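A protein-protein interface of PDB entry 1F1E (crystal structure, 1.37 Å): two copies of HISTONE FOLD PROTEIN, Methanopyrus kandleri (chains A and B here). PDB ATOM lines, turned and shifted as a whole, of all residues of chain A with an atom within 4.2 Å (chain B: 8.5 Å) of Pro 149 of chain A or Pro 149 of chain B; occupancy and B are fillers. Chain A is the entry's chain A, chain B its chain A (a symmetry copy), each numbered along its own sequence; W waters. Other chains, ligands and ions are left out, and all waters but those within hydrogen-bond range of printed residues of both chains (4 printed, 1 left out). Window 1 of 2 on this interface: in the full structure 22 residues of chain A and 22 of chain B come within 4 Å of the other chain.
The backbone carbonyl oxygen of Val 69 of chain B lies within hydrogen-bond range of the side-chain hydroxyl of Tyr 41 of chain A (2.7 Å). The backbone NH (N) of Gly 151 of chain B lies within hydrogen-bond range of the backbone carbonyl oxygen (O) of Tyr 146 of chain A. The backbone NH (N) of Lys 150 of chain B is in hydrogen-bond range of the backbone carbonyl oxygen (O) of Ser 147 of chain A, 2.8 Å away. The backbone carbonyl oxygen of Ser 147 of chain B lies within hydrogen-bond range of the backbone NH of Lys 150 of chain A (2.8 Å). The backbone carbonyl oxygen of Tyr 146 of chain B sits at hydrogen-bond distance from the backbone NH of Gly 151 of chain A, at 2.8 Å. The backbone carbonyl oxygen of Tyr 146 of chain A sits close to the backbone carbonyl oxygen of Thr 145 of chain B. O of Met 148 of chain B sits close to O of Tyr 146 of chain A (3.4 Å). O of Met 148 of chain A sits close to O of Tyr 146 of chain B, at 3.4 Å. The backbone carbonyl oxygen (O) of Met 148 of chain A lies close to the backbone carbonyl oxygen (O) of Met 148 of chain B, at 3.2 Å.
O of Ala 143 of chain B sits at hydrogen-bond distance from OG of Ser 147 of chain B (2.7 Å). OG1 of Thr 145 of chain B sits close to O of Gly 151 of chain B (3.5 Å).
Among the printed residues, merely in contact across the chains: Met 71 of chain A with Pro 149 of chain B, Met 71 of chain A with Lys 150 of chain B, Met 71 of chain A with Leu 154 of chain B, Tyr 146 of chain A with Lys 150 of chain B, Tyr 146 of chain A with Glu 153 of chain B, Ser 147 of chain A with Pro 149 of chain B, Met 148 of chain A with Pro 149 of chain B, Pro 149 of chain A with Met 71 of chain B, Pro 149 of chain A with Ser 147 of chain B, Pro 149 of chain A with Met 148 of chain B, Pro 149 of chain A with Pro 149 of chain B, Lys 150 of chain A with Leu 70 of chain B, Lys 150 of chain A with Met 71 of chain B, Lys 150 of chain A with Tyr 146 of chain B, Glu 153 of chain A with Tyr 146 of chain B and Leu 154 of chain A with Met 71 of chain B.
Printed residues of chain B within 4 Å of Pro 149 of chain A: Met 71, Ser 147, Met 148 and Pro 149. Printed residues of chain A within 4 Å of Leu 70 of chain B: Lys 150. Printed residues of chain A within 4 Å of Met 71 of chain B: Pro 149 (3.4 Å), Lys 150 (2.8 Å) and Leu 154 (3.5 Å). Ala 143 of chain B touches none of the printed residues of chain A. Printed residues of chain A within 4 Å of Tyr 146 of chain B: Met 148 (3.4 Å), Lys 150 (3.7 Å), Gly 151 (2.8 Å) and Glu 153 (3.5 Å). Of the printed residues of chain A, Leu 154 of chain B touches Met 71 (3.5 Å).
Printed residues of chain B that touch a printed residue of chain A: Val 69, Leu 70, Met 71, Thr 145, Tyr 146, Ser 147, Met 148, Pro 149, Lys 150, Gly 151, Glu 153 and Leu 154. Hydrophobic or aromatic side chains of chain B within 4 Å of the printed part of chain A: Val 69, Met 71, Tyr 146, Pro 149 and Leu 154. Of the 11 printed residues of chain A, 10 touch a printed residue of chain B. Hydrophobic or aromatic side chains of chain A that line the printed part of chain B: Tyr 41, Met 71, Tyr 146, Pro 149 and Leu 154. Among the printed residues, no Asp or Glu carboxylate lies within 4 Å of a Lys or Arg side-chain nitrogen of the other chain.
Met 71 of chain A touches Leu 154 of chain B, and with the chains exchanged Leu 154 of chain A touches Met 71 of chain B. Tyr 146 of chain A touches Lys 150 of chain B, and with the chains exchanged Lys 150 of chain A touches Tyr 146 of chain B. Tyr 146 of chain A touches Glu 153 of chain B, and with the chains exchanged Glu 153 of chain A touches Tyr 146 of chain B. Met 148 of chain A touches Pro 149 of chain B, and with the chains exchanged Pro 149 of chain A touches Met 148 of chain B. Positions printed for both chains: 41, 71, 146, 147, 148, 149, 150, 151, 152, 153 and 154.
Water W3 lies within hydrogen-bond range of O of Leu 70 of chain B (2.6 Å), O of Ser 147 of chain B (3.1 Å) and NZ of Lys 150 of chain A (3.2 Å). Water W1 lies within hydrogen-bond range of OXT of Leu 154 of chain A and SD of Met 71 of chain B. Water W4 bridges OXT of Leu 154 of chain B and SD of Met 71 of chain A. Water W2 bridges O of Ser 147 of chain A (3.1 Å) and NZ of Lys 150 of chain B (3.2 Å).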
ATOM      1  N   TYR A  41      12.755  -2.746  -4.402  1.00  0.00           N
ATOM      2  CA  TYR A  41      11.374  -3.102  -4.459  1.00  0.00           C
ATOM      3  C   TYR A  41      10.637  -2.605  -3.211  1.00  0.00           C
ATOM      4  O   TYR A  41       9.570  -2.036  -3.254  1.00  0.00           O
ATOM      5  CB  TYR A  41      11.256  -4.632  -4.636  1.00  0.00           C
ATOM      6  CG  TYR A  41       9.889  -5.135  -4.230  1.00  0.00           C
ATOM      7  CD1 TYR A  41       8.753  -5.075  -5.004  1.00  0.00           C
ATOM      8  CD2 TYR A  41       9.745  -5.739  -3.002  1.00  0.00           C
ATOM      9  CE1 TYR A  41       7.565  -5.570  -4.535  1.00  0.00           C
ATOM     10  CE2 TYR A  41       8.552  -6.241  -2.503  1.00  0.00           C
ATOM     11  CZ  TYR A  41       7.449  -6.145  -3.316  1.00  0.00           C
ATOM     12  OH  TYR A  41       6.243  -6.645  -2.843  1.00  0.00           O
ATOM     13  N   MET A  71       4.562 -10.076   5.079  1.00  0.00           N
ATOM     14  CA  MET A  71       4.539 -11.110   6.121  1.00  0.00           C
ATOM     15  C   MET A  71       5.975 -11.408   6.595  1.00  0.00           C
ATOM     16  O   MET A  71       6.342 -12.496   6.946  1.00  0.00           O
ATOM     17  CB  MET A  71       3.797 -12.359   5.767  1.00  0.00           C
ATOM     18  CG  MET A  71       2.276 -12.097   5.523  1.00  0.00           C
ATOM     19  SD  MET A  71       1.579 -13.566   4.677  1.00  0.00           S
ATOM     20  CE  MET A  71       2.362 -13.274   3.076  1.00  0.00           C
ATOM     21  N   TYR A 146       9.780 -18.880  -3.265  1.00  0.00           N
ATOM     22  CA  TYR A 146       8.717 -19.265  -2.363  1.00  0.00           C
ATOM     23  C   TYR A 146       8.308 -18.024  -1.613  1.00  0.00           C
ATOM     24  O   TYR A 146       7.153 -17.623  -1.582  1.00  0.00           O
ATOM     25  CB  TYR A 146       9.216 -20.369  -1.449  1.00  0.00           C
ATOM     26  CG  TYR A 146       8.172 -20.951  -0.561  1.00  0.00           C
ATOM     27  CD1 TYR A 146       7.867 -20.328   0.658  1.00  0.00           C
ATOM     28  CD2 TYR A 146       7.486 -22.132  -0.863  1.00  0.00           C
ATOM     29  CE1 TYR A 146       6.919 -20.826   1.514  1.00  0.00           C
ATOM     30  CE2 TYR A 146       6.519 -22.637  -0.035  1.00  0.00           C
ATOM     31  CZ  TYR A 146       6.256 -21.978   1.142  1.00  0.00           C
ATOM     32  OH  TYR A 146       5.325 -22.476   1.990  1.00  0.00           O
ATOM     33  N   SER A 147       9.290 -17.382  -0.963  1.00  0.00           N
ATOM     34  CA  SER A 147       8.924 -16.354  -0.038  1.00  0.00           C
ATOM     35  C   SER A 147       8.459 -15.020  -0.611  1.00  0.00           C
ATOM     36  O   SER A 147       7.756 -14.299   0.097  1.00  0.00           O
ATOM     37  CB  SER A 147      10.060 -16.145   0.957  1.00  0.00           C
ATOM     38  OG  SER A 147      11.133 -15.492   0.356  1.00  0.00           O
ATOM     39  N   MET A 148       8.812 -14.669  -1.821  1.00  0.00           N
ATOM     40  CA  MET A 148       8.508 -13.365  -2.366  1.00  0.00           C
ATOM     41  C   MET A 148       7.340 -13.442  -3.358  1.00  0.00           C
ATOM     42  O   MET A 148       7.070 -14.464  -3.985  1.00  0.00           O
ATOM     43  CB  MET A 148       9.772 -12.792  -3.050  1.00  0.00           C
ATOM     44  CG  MET A 148      10.864 -12.341  -2.128  1.00  0.00           C
ATOM     45  SD  MET A 148      10.594 -10.801  -1.187  1.00  0.00           S
ATOM     46  CE  MET A 148      10.674 -11.569   0.464  1.00  0.00           C
ATOM     47  N   PRO A 149       6.661 -12.346  -3.578  1.00  0.00           N
ATOM     48  CA  PRO A 149       5.654 -12.298  -4.633  1.00  0.00           C
ATOM     49  C   PRO A 149       6.335 -12.434  -5.988  1.00  0.00           C
ATOM     50  O   PRO A 149       7.460 -12.045  -6.179  1.00  0.00           O
ATOM     51  CB  PRO A 149       5.072 -10.901  -4.433  1.00  0.00           C
ATOM     52  CG  PRO A 149       6.220 -10.139  -3.834  1.00  0.00           C
ATOM     53  CD  PRO A 149       6.839 -11.076  -2.847  1.00  0.00           C
ATOM     54  N   LYS A 150       5.585 -12.934  -6.937  1.00  0.00           N
ATOM     55  CA  LYS A 150       6.044 -13.033  -8.335  1.00  0.00           C
ATOM     56  C   LYS A 150       7.370 -13.769  -8.390  1.00  0.00           C
ATOM     57  O   LYS A 150       8.227 -13.450  -9.218  1.00  0.00           O
ATOM     58  CB  LYS A 150       6.067 -11.659  -9.017  1.00  0.00           C
ATOM     59  CG  LYS A 150       4.673 -11.133  -9.204  1.00  0.00           C
ATOM     60  CD  LYS A 150       3.904 -11.884 -10.298  1.00  0.00           C
ATOM     61  CE  LYS A 150       2.607 -11.026 -10.285  1.00  0.00           C
ATOM     62  NZ  LYS A 150       1.549 -11.935 -10.582  1.00  0.00           N
ATOM     63  N   GLY A 151       7.529 -14.765  -7.536  1.00  0.00           N
ATOM     64  CA  GLY A 151       8.696 -15.611  -7.544  1.00  0.00           C
ATOM     65  C   GLY A 151       9.959 -14.874  -7.225  1.00  0.00           C
ATOM     66  O   GLY A 151      11.058 -15.295  -7.514  1.00  0.00           O
ATOM     67  N   GLY A 152       9.855 -13.700  -6.645  1.00  0.00           N
ATOM     68  CA  GLY A 152      11.056 -12.920  -6.359  1.00  0.00           C
ATOM     69  C   GLY A 152      11.537 -12.181  -7.566  1.00  0.00           C
ATOM     70  O   GLY A 152      12.643 -11.656  -7.448  1.00  0.00           O
ATOM     71  N   GLU A 153      10.805 -12.095  -8.643  1.00  0.00           N
ATOM     72  CA  GLU A 153      11.213 -11.287  -9.778  1.00  0.00           C
ATOM     73  C   GLU A 153      10.833  -9.841  -9.571  1.00  0.00           C
ATOM     74  O   GLU A 153       9.916  -9.290 -10.148  1.00  0.00           O
ATOM     75  CB  GLU A 153      10.607 -11.948 -11.031  1.00  0.00           C
ATOM     76  CG  GLU A 153      11.181 -13.331 -11.196  1.00  0.00           C
ATOM     77  CD  GLU A 153      11.126 -13.916 -12.593  1.00  0.00           C
ATOM     78  OE1 GLU A 153      10.171 -13.538 -13.342  1.00  0.00           O
ATOM     79  OE2 GLU A 153      12.022 -14.725 -12.917  1.00  0.00           O
ATOM     80  N   LEU A 154      11.555  -9.273  -8.626  1.00  0.00           N
ATOM     81  CA  LEU A 154      11.274  -7.975  -8.059  1.00  0.00           C
ATOM     82  C   LEU A 154      12.028  -6.839  -8.734  1.00  0.00           C
ATOM     83  O   LEU A 154      12.903  -7.184  -9.566  1.00  0.00           O
ATOM     84  CB  LEU A 154      11.656  -7.939  -6.554  1.00  0.00           C
ATOM     85  CG  LEU A 154      11.084  -8.976  -5.666  1.00  0.00           C
ATOM     86  CD1 LEU A 154      11.610  -8.799  -4.219  1.00  0.00           C
ATOM     87  CD2 LEU A 154       9.539  -9.018  -5.708  1.00  0.00           C
ATOM     88  OXT LEU A 154      11.675  -5.674  -8.399  1.00  0.00           O
ATOM     89  N   PHE B  34      -8.006 -21.477  -1.549  1.00  0.00           N
ATOM     90  CA  PHE B  34      -7.093 -20.370  -1.595  1.00  0.00           C
ATOM     91  C   PHE B  34      -7.711 -18.986  -1.848  1.00  0.00           C
ATOM     92  O   PHE B  34      -7.357 -18.032  -1.173  1.00  0.00           O
ATOM     93  CB  PHE B  34      -6.022 -20.667  -2.673  1.00  0.00           C
ATOM     94  CG  PHE B  34      -5.102 -19.476  -2.831  1.00  0.00           C
ATOM     95  CD1 PHE B  34      -4.110 -19.290  -1.864  1.00  0.00           C
ATOM     96  CD2 PHE B  34      -5.209 -18.644  -3.922  1.00  0.00           C
ATOM     97  CE1 PHE B  34      -3.274 -18.210  -2.024  1.00  0.00           C
ATOM     98  CE2 PHE B  34      -4.401 -17.522  -4.021  1.00  0.00           C
ATOM     99  CZ  PHE B  34      -3.437 -17.367  -3.078  1.00  0.00           C
ATOM    100  N   MET B  38      -6.877 -15.585   0.085  1.00  0.00           N
ATOM    101  CA  MET B  38      -6.239 -14.467  -0.593  1.00  0.00           C
ATOM    102  C   MET B  38      -7.070 -13.207  -0.500  1.00  0.00           C
ATOM    103  O   MET B  38      -6.537 -12.141  -0.243  1.00  0.00           O
ATOM    104  CB  MET B  38      -5.945 -14.819  -2.047  1.00  0.00           C
ATOM    105  CG  MET B  38      -5.316 -13.711  -2.809  1.00  0.00           C
ATOM    106  SD  MET B  38      -6.464 -12.553  -3.597  1.00  0.00           S
ATOM    107  CE  MET B  38      -7.258 -13.555  -4.830  1.00  0.00           C
ATOM    108  N   TYR B  41      -6.618 -11.828   2.957  1.00  0.00           N
ATOM    109  CA  TYR B  41      -5.293 -11.309   3.068  1.00  0.00           C
ATOM    110  C   TYR B  41      -5.207  -9.913   2.444  1.00  0.00           C
ATOM    111  O   TYR B  41      -4.656  -8.979   2.982  1.00  0.00           O
ATOM    112  CB  TYR B  41      -4.308 -12.303   2.414  1.00  0.00           C
ATOM    113  CG  TYR B  41      -2.997 -11.636   2.062  1.00  0.00           C
ATOM    114  CD1 TYR B  41      -1.970 -11.377   2.941  1.00  0.00           C
ATOM    115  CD2 TYR B  41      -2.769 -11.276   0.753  1.00  0.00           C
ATOM    116  CE1 TYR B  41      -0.821 -10.772   2.509  1.00  0.00           C
ATOM    117  CE2 TYR B  41      -1.617 -10.657   0.294  1.00  0.00           C
ATOM    118  CZ  TYR B  41      -0.630 -10.415   1.218  1.00  0.00           C
ATOM    119  OH  TYR B  41       0.537  -9.799   0.782  1.00  0.00           O
ATOM    120  N   LEU B  66      -1.541  -1.570  -3.052  1.00  0.00           N
ATOM    121  CA  LEU B  66      -1.414  -2.988  -2.828  1.00  0.00           C
ATOM    122  C   LEU B  66      -1.141  -3.697  -4.149  1.00  0.00           C
ATOM    123  O   LEU B  66      -0.384  -4.646  -4.218  1.00  0.00           O
ATOM    124  CB  LEU B  66      -2.664  -3.661  -2.231  1.00  0.00           C
ATOM    125  CG  LEU B  66      -3.084  -3.503  -0.795  1.00  0.00           C
ATOM    126  CD1 LEU B  66      -4.346  -4.288  -0.557  1.00  0.00           C
ATOM    127  CD2 LEU B  66      -1.934  -3.914   0.128  1.00  0.00           C
ATOM    128  N   ALA B  67      -1.831  -3.297  -5.190  1.00  0.00           N
ATOM    129  CA  ALA B  67      -1.582  -3.918  -6.504  1.00  0.00           C
ATOM    130  C   ALA B  67      -0.152  -3.721  -6.937  1.00  0.00           C
ATOM    131  O   ALA B  67       0.388  -4.689  -7.474  1.00  0.00           O
ATOM    132  CB  ALA B  67      -2.511  -3.380  -7.566  1.00  0.00           C
ATOM    133  N   ASP B  68       0.381  -2.536  -6.655  1.00  0.00           N
ATOM    134  CA  ASP B  68       1.759  -2.239  -7.114  1.00  0.00           C
ATOM    135  C   ASP B  68       2.627  -3.112  -6.256  1.00  0.00           C
ATOM    136  O   ASP B  68       3.560  -3.831  -6.772  1.00  0.00           O
ATOM    137  CB  ASP B  68       2.004  -0.746  -7.243  1.00  0.00           C
ATOM    138  CG  ASP B  68       2.272   0.349  -6.254  1.00  0.00           C
ATOM    139  N   VAL B  69       2.421  -3.313  -4.953  1.00  0.00           N
ATOM    140  CA  VAL B  69       3.369  -4.146  -4.230  1.00  0.00           C
ATOM    141  C   VAL B  69       3.185  -5.653  -4.442  1.00  0.00           C
ATOM    142  O   VAL B  69       4.129  -6.448  -4.443  1.00  0.00           O
ATOM    143  CB  VAL B  69       3.479  -3.908  -2.706  1.00  0.00           C
ATOM    144  CG1 VAL B  69       3.155  -2.461  -2.316  1.00  0.00           C
ATOM    145  CG2 VAL B  69       2.650  -4.982  -2.008  1.00  0.00           C
ATOM    146  N   LEU B  70       1.963  -6.140  -4.675  1.00  0.00           N
ATOM    147  CA  LEU B  70       1.800  -7.536  -5.044  1.00  0.00           C
ATOM    148  C   LEU B  70       2.149  -7.807  -6.508  1.00  0.00           C
ATOM    149  O   LEU B  70       2.188  -8.999  -6.899  1.00  0.00           O
ATOM    150  CB  LEU B  70       0.340  -7.966  -4.786  1.00  0.00           C
ATOM    151  CG  LEU B  70      -0.039  -7.878  -3.298  1.00  0.00           C
ATOM    152  CD1 LEU B  70      -1.527  -8.078  -3.120  1.00  0.00           C
ATOM    153  CD2 LEU B  70       0.748  -8.946  -2.531  1.00  0.00           C
ATOM    154  N   MET B  71       2.356  -6.767  -7.270  1.00  0.00           N
ATOM    155  CA  MET B  71       2.760  -6.846  -8.679  1.00  0.00           C
ATOM    156  C   MET B  71       1.680  -7.585  -9.494  1.00  0.00           C
ATOM    157  O   MET B  71       1.929  -8.288 -10.436  1.00  0.00           O
ATOM    158  CB  MET B  71       4.125  -7.409  -8.922  1.00  0.00           C
ATOM    159  CG  MET B  71       5.251  -6.522  -8.300  1.00  0.00           C
ATOM    160  SD  MET B  71       6.793  -7.512  -8.263  1.00  0.00           S
ATOM    161  CE  MET B  71       6.293  -8.626  -6.933  1.00  0.00           C
ATOM    162  N   VAL B  72       0.417  -7.340  -9.178  1.00  0.00           N
ATOM    163  CA  VAL B  72      -0.690  -7.855  -9.964  1.00  0.00           C
ATOM    164  C   VAL B  72      -0.855  -6.949 -11.183  1.00  0.00           C
ATOM    165  O   VAL B  72      -0.996  -5.709 -11.066  1.00  0.00           O
ATOM    166  CB  VAL B  72      -1.972  -7.882  -9.120  1.00  0.00           C
ATOM    167  CG1 VAL B  72      -3.167  -8.376  -9.891  1.00  0.00           C
ATOM    168  CG2 VAL B  72      -1.775  -8.784  -7.878  1.00  0.00           C
ATOM    169  N   ALA B 143       1.557 -22.370  -8.815  1.00  0.00           N
ATOM    170  CA  ALA B 143       1.233 -20.988  -9.099  1.00  0.00           C
ATOM    171  C   ALA B 143       1.065 -20.128  -7.849  1.00  0.00           C
ATOM    172  O   ALA B 143       1.548 -18.984  -7.776  1.00  0.00           O
ATOM    173  CB  ALA B 143      -0.016 -20.910  -9.968  1.00  0.00           C
ATOM    174  N   ILE B 144       0.412 -20.695  -6.821  1.00  0.00           N
ATOM    175  CA  ILE B 144       0.272 -20.014  -5.536  1.00  0.00           C
ATOM    176  C   ILE B 144       1.611 -19.754  -4.903  1.00  0.00           C
ATOM    177  O   ILE B 144       1.853 -18.629  -4.475  1.00  0.00           O
ATOM    178  CB  ILE B 144      -0.691 -20.838  -4.671  1.00  0.00           C
ATOM    179  CG1 ILE B 144      -2.138 -20.809  -5.144  1.00  0.00           C
ATOM    180  CG2 ILE B 144      -0.600 -20.408  -3.242  1.00  0.00           C
ATOM    181  CD1 ILE B 144      -3.049 -21.868  -4.575  1.00  0.00           C
ATOM    182  N   THR B 145       2.415 -20.817  -4.834  1.00  0.00           N
ATOM    183  CA  THR B 145       3.668 -20.667  -4.088  1.00  0.00           C
ATOM    184  C   THR B 145       4.565 -19.651  -4.766  1.00  0.00           C
ATOM    185  O   THR B 145       5.190 -18.826  -4.114  1.00  0.00           O
ATOM    186  CB  THR B 145       4.331 -22.043  -4.031  1.00  0.00           C
ATOM    187  OG1 THR B 145       3.654 -22.835  -3.075  1.00  0.00           O
ATOM    188  CG2 THR B 145       5.743 -21.806  -3.582  1.00  0.00           C
ATOM    189  N   TYR B 146       4.615 -19.723  -6.094  1.00  0.00           N
ATOM    190  CA  TYR B 146       5.523 -18.886  -6.847  1.00  0.00           C
ATOM    191  C   TYR B 146       5.019 -17.472  -6.722  1.00  0.00           C
ATOM    192  O   TYR B 146       5.721 -16.555  -6.319  1.00  0.00           O
ATOM    193  CB  TYR B 146       5.570 -19.371  -8.284  1.00  0.00           C
ATOM    194  CG  TYR B 146       6.575 -18.676  -9.135  1.00  0.00           C
ATOM    195  CD1 TYR B 146       6.247 -17.457  -9.747  1.00  0.00           C
ATOM    196  CD2 TYR B 146       7.846 -19.198  -9.394  1.00  0.00           C
ATOM    197  CE1 TYR B 146       7.133 -16.780 -10.545  1.00  0.00           C
ATOM    198  CE2 TYR B 146       8.757 -18.531 -10.168  1.00  0.00           C
ATOM    199  CZ  TYR B 146       8.383 -17.335 -10.734  1.00  0.00           C
ATOM    200  OH  TYR B 146       9.257 -16.672 -11.528  1.00  0.00           O
ATOM    201  N   SER B 147       3.746 -17.267  -7.094  1.00  0.00           N
ATOM    202  CA  SER B 147       3.295 -15.918  -7.235  1.00  0.00           C
ATOM    203  C   SER B 147       3.029 -15.124  -5.962  1.00  0.00           C
ATOM    204  O   SER B 147       3.062 -13.895  -6.027  1.00  0.00           O
ATOM    205  CB  SER B 147       2.077 -15.888  -8.151  1.00  0.00           C
ATOM    206  OG  SER B 147       0.956 -16.401  -7.504  1.00  0.00           O
ATOM    207  N   MET B 148       2.771 -15.750  -4.842  1.00  0.00           N
ATOM    208  CA  MET B 148       2.386 -15.050  -3.637  1.00  0.00           C
ATOM    209  C   MET B 148       3.555 -14.977  -2.647  1.00  0.00           C
ATOM    210  O   MET B 148       4.462 -15.807  -2.629  1.00  0.00           O
ATOM    211  CB  MET B 148       1.170 -15.765  -2.999  1.00  0.00           C
ATOM    212  CG  MET B 148      -0.134 -15.597  -3.718  1.00  0.00           C
ATOM    213  SD  MET B 148      -0.953 -13.970  -3.616  1.00  0.00           S
ATOM    214  CE  MET B 148      -0.892 -13.612  -5.402  1.00  0.00           C
ATOM    215  N   PRO B 149       3.530 -14.024  -1.751  1.00  0.00           N
ATOM    216  CA  PRO B 149       4.511 -13.996  -0.671  1.00  0.00           C
ATOM    217  C   PRO B 149       4.287 -15.191   0.245  1.00  0.00           C
ATOM    218  O   PRO B 149       3.196 -15.678   0.404  1.00  0.00           O
ATOM    219  CB  PRO B 149       4.161 -12.682   0.022  1.00  0.00           C
ATOM    220  CG  PRO B 149       2.697 -12.522  -0.274  1.00  0.00           C
ATOM    221  CD  PRO B 149       2.539 -12.930  -1.703  1.00  0.00           C
ATOM    222  N   LYS B 150       5.348 -15.596   0.896  1.00  0.00           N
ATOM    223  CA  LYS B 150       5.291 -16.666   1.910  1.00  0.00           C
ATOM    224  C   LYS B 150       4.643 -17.903   1.314  1.00  0.00           C
ATOM    225  O   LYS B 150       3.925 -18.626   2.009  1.00  0.00           O
ATOM    226  CB  LYS B 150       4.628 -16.179   3.204  1.00  0.00           C
ATOM    227  CG  LYS B 150       5.494 -15.166   3.898  1.00  0.00           C
ATOM    228  CD  LYS B 150       6.737 -15.796   4.537  1.00  0.00           C
ATOM    229  CE  LYS B 150       7.301 -14.522   5.227  1.00  0.00           C
ATOM    230  NZ  LYS B 150       8.720 -14.661   5.178  1.00  0.00           N
ATOM    231  N   GLY B 151       4.915 -18.161   0.047  1.00  0.00           N
ATOM    232  CA  GLY B 151       4.449 -19.352  -0.616  1.00  0.00           C
ATOM    233  C   GLY B 151       2.957 -19.425  -0.716  1.00  0.00           C
ATOM    234  O   GLY B 151       2.358 -20.461  -0.907  1.00  0.00           O
ATOM    235  N   GLY B 152       2.276 -18.314  -0.544  1.00  0.00           N
ATOM    236  CA  GLY B 152       0.816 -18.342  -0.581  1.00  0.00           C
ATOM    237  C   GLY B 152       0.237 -18.794   0.720  1.00  0.00           C
ATOM    238  O   GLY B 152      -0.973 -19.019   0.701  1.00  0.00           O
ATOM    239  N   GLU B 153       0.978 -18.908   1.787  1.00  0.00           N
ATOM    240  CA  GLU B 153       0.406 -19.236   3.081  1.00  0.00           C
ATOM    241  C   GLU B 153      -0.136 -18.000   3.756  1.00  0.00           C
ATOM    242  O   GLU B 153       0.402 -17.450   4.697  1.00  0.00           O
ATOM    243  CB  GLU B 153       1.497 -19.986   3.869  1.00  0.00           C
ATOM    244  CG  GLU B 153       1.838 -21.269   3.156  1.00  0.00           C
ATOM    245  CD  GLU B 153       2.468 -22.357   4.001  1.00  0.00           C
ATOM    246  OE1 GLU B 153       3.166 -21.986   4.997  1.00  0.00           O
ATOM    247  OE2 GLU B 153       2.258 -23.544   3.668  1.00  0.00           O
ATOM    248  N   LEU B 154      -1.212 -17.540   3.151  1.00  0.00           N
ATOM    249  CA  LEU B 154      -1.817 -16.259   3.433  1.00  0.00           C
ATOM    250  C   LEU B 154      -2.937 -16.328   4.459  1.00  0.00           C
ATOM    251  O   LEU B 154      -3.297 -17.483   4.798  1.00  0.00           O
ATOM    252  CB  LEU B 154      -2.424 -15.643   2.143  1.00  0.00           C
ATOM    253  CG  LEU B 154      -1.544 -15.499   0.961  1.00  0.00           C
ATOM    254  CD1 LEU B 154      -2.335 -14.905  -0.233  1.00  0.00           C
ATOM    255  CD2 LEU B 154      -0.266 -14.682   1.258  1.00  0.00           C
ATOM    256  OXT LEU B 154      -3.368 -15.215   4.875  1.00  0.00           O
HETATM  257  O   HOH W   1       9.065  -4.857  -8.338  1.00  0.00           O
HETATM  258  O   HOH W   2       7.852 -12.734   2.744  1.00  0.00           O
HETATM  259  O   HOH W   3       1.619 -11.540  -7.383  1.00  0.00           O
HETATM  260  O   HOH W   4      -1.729 -13.205   5.745  1.00  0.00           O
